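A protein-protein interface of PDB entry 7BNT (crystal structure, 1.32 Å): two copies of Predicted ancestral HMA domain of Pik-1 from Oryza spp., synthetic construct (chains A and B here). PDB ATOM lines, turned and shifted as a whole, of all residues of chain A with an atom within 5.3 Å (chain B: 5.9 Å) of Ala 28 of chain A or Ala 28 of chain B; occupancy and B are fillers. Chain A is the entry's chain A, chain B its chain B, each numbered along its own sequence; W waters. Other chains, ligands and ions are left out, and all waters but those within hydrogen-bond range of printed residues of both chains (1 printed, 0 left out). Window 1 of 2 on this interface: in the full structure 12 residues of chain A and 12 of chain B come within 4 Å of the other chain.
The side-chain hydroxyl (OG) of Ser 21 of chain A lies within hydrogen-bond range of the backbone carbonyl oxygen (O) of Ser 29 of chain B, at 2.8 Å.
N of Val 36 of chain B lies within hydrogen-bond range of O of Val 36 of chain A (2.9 Å).
O of Ala 28 of chain B touches CB of Met 24 of chain A, at 3.4 Å.
O of Ala 25 of chain A touches CB of Ala 25 of chain B, 3.5 Å away.
Ala 25 of chain A touches Ser 29 of chain B.
Ala 28 of chain A touches Ser 21 of chain B (O to O, 3.9 Å).
O of Ala 28 of chain A touches CB of Met 24 of chain B, 3.5 Å away.
Ala 28 of chain A touches Ala 25 of chain B (CB to N, 3.996 Å).
Ala 28 of chain B touches Ala 28 of chain A (CB to CB, 3.5 Å).
Ser 29 of chain A touches Ser 21 of chain B (O to CB, 3.6 Å).
Ala 25 of chain B touches Ser 29 of chain A (CB to CB, 3.9 Å).
Water W1 lies within hydrogen-bond range of the backbone carbonyl oxygen (O) of Ala 28 of chain A, the backbone carbonyl oxygen (O) of Thr 30 of chain A and the side-chain hydroxyl (OG) of Ser 21 of chain B.
Ser 21 of chain A touches Ser 29 of chain B, and with the chains exchanged Ser 29 of chain A touches Ser 21 of chain B.
Met 24 of chain A touches Ala 28 of chain B, and with the chains exchanged Ala 28 of chain A touches Met 24 of chain B.
Ala 28 of chain A touches Ala 25 of chain B, but with the chains exchanged Ala 25 of chain A does not touch Ala 28 of chain B (4.4 Å).
Val 36 of chain A touches its own counterpart, Val 36 of chain B.
Printed residues of chain B within 4 Å of Ala 28 of chain A: Ser 21 (3.9 Å), Met 24 (3.5 Å), Ala 25 (3.996 Å) and Ala 28 (3.5 Å).
Of chain A, only Met 24 and Ala 28 come within 4 Å of Ala 28 of chain B.
Of the printed residues of chain B, Val 36 of chain A touches Val 36.
Of the printed residues of chain A, Ser 29 of chain B touches Ser 21 (2.8 Å) and Ala 25 (3.9 Å).
Of the printed residues of chain B, Ser 21 of chain A touches Ser 29.
Printed residues of chain A within 4 Å of Ala 25 of chain B: Ala 25, Ala 28 and Ser 29.
The nearest printed residue of chain B that does not touch Ala 28 of chain A is Val 36 of chain B (4.7 Å).
The nearest residue of chain A that does not touch Ala 28 of chain B is Ala 25 of chain A (4.4 Å).
Printed residues of chain A that touch a printed residue of chain B: Ser 21, Met 24, Ala 25, Ala 28, Ser 29 and Val 36.
Hydrophobic or aromatic side chains of chain A that line the printed part of chain B: Met 24, Ala 25 and Ala 28.
Hydrophobic or aromatic side chains of chain B within 4 Å of the printed part of chain A: Met 24, Ala 25, Ala 28 and Val 36.
The backbone carbonyl oxygen (O) of Ala 25 of chain A sits close to the side-chain hydroxyl (OG) of Ser 29 of chain A, 3.5 Å away.
The backbone carbonyl oxygen of Leu 26 of chain A is in hydrogen-bond range of the side-chain hydroxyl of Ser 29 of chain A.
The side-chain hydroxyl (OG) of Ser 29 of chain B sits at hydrogen-bond distance from the backbone carbonyl oxygen (O) of Leu 26 of chain B (2.8 Å).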
ATOM      1  N   SER A  21       6.593  31.050   1.213  1.00  0.00           N
ATOM      2  CA  SER A  21       5.811  29.810   1.432  1.00  0.00           C
ATOM      3  C   SER A  21       6.076  29.286   2.844  1.00  0.00           C
ATOM      4  O   SER A  21       5.121  28.974   3.563  1.00  0.00           O
ATOM      5  CB  SER A  21       6.197  28.820   0.385  1.00  0.00           C
ATOM      6  OG  SER A  21       5.590  27.580   0.603  1.00  0.00           O
ATOM      7  N   ALA A  23       7.265  30.894   5.490  1.00  0.00           N
ATOM      8  CA  ALA A  23       6.850  31.855   6.521  1.00  0.00           C
ATOM      9  C   ALA A  23       5.334  31.809   6.650  1.00  0.00           C
ATOM     10  O   ALA A  23       4.832  31.755   7.791  1.00  0.00           O
ATOM     11  CB  ALA A  23       7.322  33.225   6.137  1.00  0.00           C
ATOM     12  N   MET A  24       4.637  31.798   5.520  1.00  0.00           N
ATOM     13  CA  MET A  24       3.164  31.761   5.553  1.00  0.00           C
ATOM     14  C   MET A  24       2.691  30.449   6.174  1.00  0.00           C
ATOM     15  O   MET A  24       1.750  30.480   6.981  1.00  0.00           O
ATOM     16  CB  MET A  24       2.596  31.942   4.145  1.00  0.00           C
ATOM     17  CG  MET A  24       2.660  33.376   3.702  1.00  0.00           C
ATOM     18  SD  MET A  24       1.502  34.445   4.616  1.00  0.00           S
ATOM     19  CE  MET A  24      -0.024  34.078   3.742  1.00  0.00           C
ATOM     20  N   ALA A  25       3.296  29.327   5.817  1.00  0.00           N
ATOM     21  CA  ALA A  25       2.923  28.009   6.367  1.00  0.00           C
ATOM     22  C   ALA A  25       3.117  28.041   7.881  1.00  0.00           C
ATOM     23  O   ALA A  25       2.229  27.577   8.586  1.00  0.00           O
ATOM     24  CB  ALA A  25       3.720  26.904   5.712  1.00  0.00           C
ATOM     25  N   LEU A  26       4.259  28.545   8.347  1.00  0.00           N
ATOM     26  CA  LEU A  26       4.560  28.533   9.791  1.00  0.00           C
ATOM     27  C   LEU A  26       3.523  29.374  10.523  1.00  0.00           C
ATOM     28  O   LEU A  26       2.939  28.915  11.514  1.00  0.00           O
ATOM     29  CB  LEU A  26       5.986  29.049   9.974  1.00  0.00           C
ATOM     30  CG  LEU A  26       6.513  29.033  11.397  1.00  0.00           C
ATOM     31  CD1 LEU A  26       8.021  29.182  11.387  1.00  0.00           C
ATOM     32  CD2 LEU A  26       5.899  30.124  12.251  1.00  0.00           C
ATOM     33  N   VAL A  27       3.287  30.597  10.052  1.00  0.00           N
ATOM     34  CA  VAL A  27       2.314  31.484  10.748  1.00  0.00           C
ATOM     35  C   VAL A  27       0.919  30.855  10.719  1.00  0.00           C
ATOM     36  O   VAL A  27       0.256  30.817  11.759  1.00  0.00           O
ATOM     37  CB  VAL A  27       2.317  32.901  10.157  1.00  0.00           C
ATOM     38  CG1 VAL A  27       1.226  33.754  10.787  1.00  0.00           C
ATOM     39  CG2 VAL A  27       3.683  33.536  10.351  1.00  0.00           C
ATOM     40  N   ALA A  28       0.488  30.342   9.577  1.00  0.00           N
ATOM     41  CA  ALA A  28      -0.891  29.848   9.414  1.00  0.00           C
ATOM     42  C   ALA A  28      -1.079  28.582  10.242  1.00  0.00           C
ATOM     43  O   ALA A  28      -2.228  28.274  10.534  1.00  0.00           O
ATOM     44  CB  ALA A  28      -1.200  29.590   7.965  1.00  0.00           C
ATOM     45  N   SER A  29       0.004  27.878  10.569  1.00  0.00           N
ATOM     46  CA  SER A  29      -0.040  26.602  11.335  1.00  0.00           C
ATOM     47  C   SER A  29      -0.216  26.890  12.828  1.00  0.00           C
ATOM     48  O   SER A  29      -0.415  25.934  13.599  1.00  0.00           O
ATOM     49  CB  SER A  29       1.200  25.776  11.076  1.00  0.00           C
ATOM     50  OG  SER A  29       2.308  26.271  11.813  1.00  0.00           O
ATOM     51  N   THR A  30      -0.049  28.147  13.243  1.00  0.00           N
ATOM     52  CA  THR A  30       0.059  28.534  14.668  1.00  0.00           C
ATOM     53  C   THR A  30      -1.302  28.409  15.354  1.00  0.00           C
ATOM     54  O   THR A  30      -2.346  28.799  14.771  1.00  0.00           O
ATOM     55  CB  THR A  30       0.693  29.918  14.811  1.00  0.00           C
ATOM     56  OG1 THR A  30       2.017  29.836  14.267  1.00  0.00           O
ATOM     57  CG2 THR A  30       0.758  30.357  16.254  1.00  0.00           C
ATOM     58  N   VAL A  33      -4.892  30.967  15.315  1.00  0.00           N
ATOM     59  CA  VAL A  33      -4.939  31.857  14.128  1.00  0.00           C
ATOM     60  C   VAL A  33      -6.329  31.853  13.484  1.00  0.00           C
ATOM     61  O   VAL A  33      -6.882  30.791  13.181  1.00  0.00           O
ATOM     62  CB  VAL A  33      -3.839  31.477  13.131  1.00  0.00           C
ATOM     63  CG1 VAL A  33      -4.056  32.146  11.786  1.00  0.00           C
ATOM     64  CG2 VAL A  33      -2.458  31.796  13.686  1.00  0.00           C
ATOM     65  N   VAL A  36      -4.425  35.094   8.056  1.00  0.00           N
ATOM     66  CA  VAL A  36      -3.035  35.463   7.694  1.00  0.00           C
ATOM     67  C   VAL A  36      -3.076  36.183   6.368  1.00  0.00           C
ATOM     68  O   VAL A  36      -3.667  35.648   5.432  1.00  0.00           O
ATOM     69  CB  VAL A  36      -2.116  34.238   7.642  1.00  0.00           C
ATOM     70  CG1 VAL A  36      -0.702  34.690   7.479  1.00  0.00           C
ATOM     71  CG2 VAL A  36      -2.272  33.339   8.858  1.00  0.00           C
ATOM     72  N   SER B  21      -5.341  23.437  11.303  1.00  0.00           N
ATOM     73  CA  SER B  21      -4.106  24.240  11.176  1.00  0.00           C
ATOM     74  C   SER B  21      -3.179  23.705  10.064  1.00  0.00           C
ATOM     75  O   SER B  21      -2.565  24.545   9.353  1.00  0.00           O
ATOM     76  CB  SER B  21      -3.421  24.308  12.502  1.00  0.00           C
ATOM     77  OG  SER B  21      -4.156  25.136  13.403  1.00  0.00           O
ATOM     78  N   ALA B  23      -4.286  22.269   7.348  1.00  0.00           N
ATOM     79  CA  ALA B  23      -4.990  22.703   6.126  1.00  0.00           C
ATOM     80  C   ALA B  23      -4.655  24.180   5.862  1.00  0.00           C
ATOM     81  O   ALA B  23      -4.334  24.535   4.730  1.00  0.00           O
ATOM     82  CB  ALA B  23      -6.470  22.471   6.244  1.00  0.00           C
ATOM     83  N   MET B  24      -4.730  25.008   6.911  1.00  0.00           N
ATOM     84  CA  MET B  24      -4.385  26.452   6.845  1.00  0.00           C
ATOM     85  C   MET B  24      -2.956  26.605   6.316  1.00  0.00           C
ATOM     86  O   MET B  24      -2.734  27.407   5.402  1.00  0.00           O
ATOM     87  CB  MET B  24      -4.523  27.116   8.219  1.00  0.00           C
ATOM     88  CG  MET B  24      -5.964  27.460   8.593  1.00  0.00           C
ATOM     89  SD  MET B  24      -6.647  28.882   7.683  1.00  0.00           S
ATOM     90  CE  MET B  24      -5.985  30.235   8.636  1.00  0.00           C
ATOM     91  N   ALA B  25      -2.025  25.838   6.866  1.00  0.00           N
ATOM     92  CA  ALA B  25      -0.601  25.906   6.490  1.00  0.00           C
ATOM     93  C   ALA B  25      -0.420  25.519   5.022  1.00  0.00           C
ATOM     94  O   ALA B  25       0.315  26.219   4.283  1.00  0.00           O
ATOM     95  CB  ALA B  25       0.231  25.012   7.367  1.00  0.00           C
ATOM     96  N   LEU B  26      -1.074  24.447   4.598  1.00  0.00           N
ATOM     97  CA  LEU B  26      -0.952  23.994   3.193  1.00  0.00           C
ATOM     98  C   LEU B  26      -1.457  25.102   2.275  1.00  0.00           C
ATOM     99  O   LEU B  26      -0.755  25.467   1.292  1.00  0.00           O
ATOM    100  CB  LEU B  26      -1.696  22.681   2.989  1.00  0.00           C
ATOM    101  CG  LEU B  26      -1.577  22.088   1.587  1.00  0.00           C
ATOM    102  CD1 LEU B  26      -1.808  20.584   1.633  1.00  0.00           C
ATOM    103  CD2 LEU B  26      -2.548  22.719   0.600  1.00  0.00           C
ATOM    104  N   VAL B  27      -2.644  25.643   2.550  1.00  0.00           N
ATOM    105  CA  VAL B  27      -3.199  26.686   1.652  1.00  0.00           C
ATOM    106  C   VAL B  27      -2.282  27.906   1.684  1.00  0.00           C
ATOM    107  O   VAL B  27      -1.928  28.420   0.612  1.00  0.00           O
ATOM    108  CB  VAL B  27      -4.644  27.027   2.018  1.00  0.00           C
ATOM    109  CG1 VAL B  27      -5.146  28.154   1.132  1.00  0.00           C
ATOM    110  CG2 VAL B  27      -5.522  25.780   1.913  1.00  0.00           C
ATOM    111  N   ALA B  28      -1.895  28.364   2.866  1.00  0.00           N
ATOM    112  CA  ALA B  28      -1.088  29.589   3.003  1.00  0.00           C
ATOM    113  C   ALA B  28       0.238  29.443   2.213  1.00  0.00           C
ATOM    114  O   ALA B  28       0.730  30.457   1.738  1.00  0.00           O
ATOM    115  CB  ALA B  28      -0.838  29.887   4.458  1.00  0.00           C
ATOM    116  N   SER B  29       0.798  28.228   2.144  1.00  0.00           N
ATOM    117  CA  SER B  29       2.087  27.821   1.530  1.00  0.00           C
ATOM    118  C   SER B  29       2.001  27.837  -0.003  1.00  0.00           C
ATOM    119  O   SER B  29       3.077  27.762  -0.648  1.00  0.00           O
ATOM    120  CB  SER B  29       2.550  26.439   2.061  1.00  0.00           C
ATOM    121  OG  SER B  29       2.007  25.339   1.314  1.00  0.00           O
ATOM    122  N   THR B  30       0.780  27.900  -0.563  1.00  0.00           N
ATOM    123  CA  THR B  30       0.524  27.684  -2.004  1.00  0.00           C
ATOM    124  C   THR B  30       0.950  28.932  -2.780  1.00  0.00           C
ATOM    125  O   THR B  30       0.685  30.051  -2.324  1.00  0.00           O
ATOM    126  CB  THR B  30      -0.946  27.275  -2.208  1.00  0.00           C
ATOM    127  OG1 THR B  30      -1.157  26.041  -1.493  1.00  0.00           O
ATOM    128  CG2 THR B  30      -1.310  27.077  -3.658  1.00  0.00           C
ATOM    129  N   VAL B  33      -0.985  32.765  -3.341  1.00  0.00           N
ATOM    130  CA  VAL B  33      -1.906  33.083  -2.222  1.00  0.00           C
ATOM    131  C   VAL B  33      -1.461  34.373  -1.550  1.00  0.00           C
ATOM    132  O   VAL B  33      -0.296  34.502  -1.175  1.00  0.00           O
ATOM    133  CB  VAL B  33      -2.008  31.911  -1.236  1.00  0.00           C
ATOM    134  CG1 VAL B  33      -2.758  32.306   0.037  1.00  0.00           C
ATOM    135  CG2 VAL B  33      -2.645  30.719  -1.938  1.00  0.00           C
ATOM    136  N   VAL B  36      -5.423  34.107   3.762  1.00  0.00           N
ATOM    137  CA  VAL B  36      -6.287  32.955   4.118  1.00  0.00           C
ATOM    138  C   VAL B  36      -7.011  33.332   5.401  1.00  0.00           C
ATOM    139  O   VAL B  36      -6.422  33.984   6.265  1.00  0.00           O
ATOM    140  CB  VAL B  36      -5.505  31.645   4.334  1.00  0.00           C
ATOM    141  CG1 VAL B  36      -4.861  31.206   3.047  1.00  0.00           C
ATOM    142  CG2 VAL B  36      -4.479  31.761   5.434  1.00  0.00           C
HETATM  143  O   HOH W   1      -3.578  27.658  12.703  1.00  0.00           O
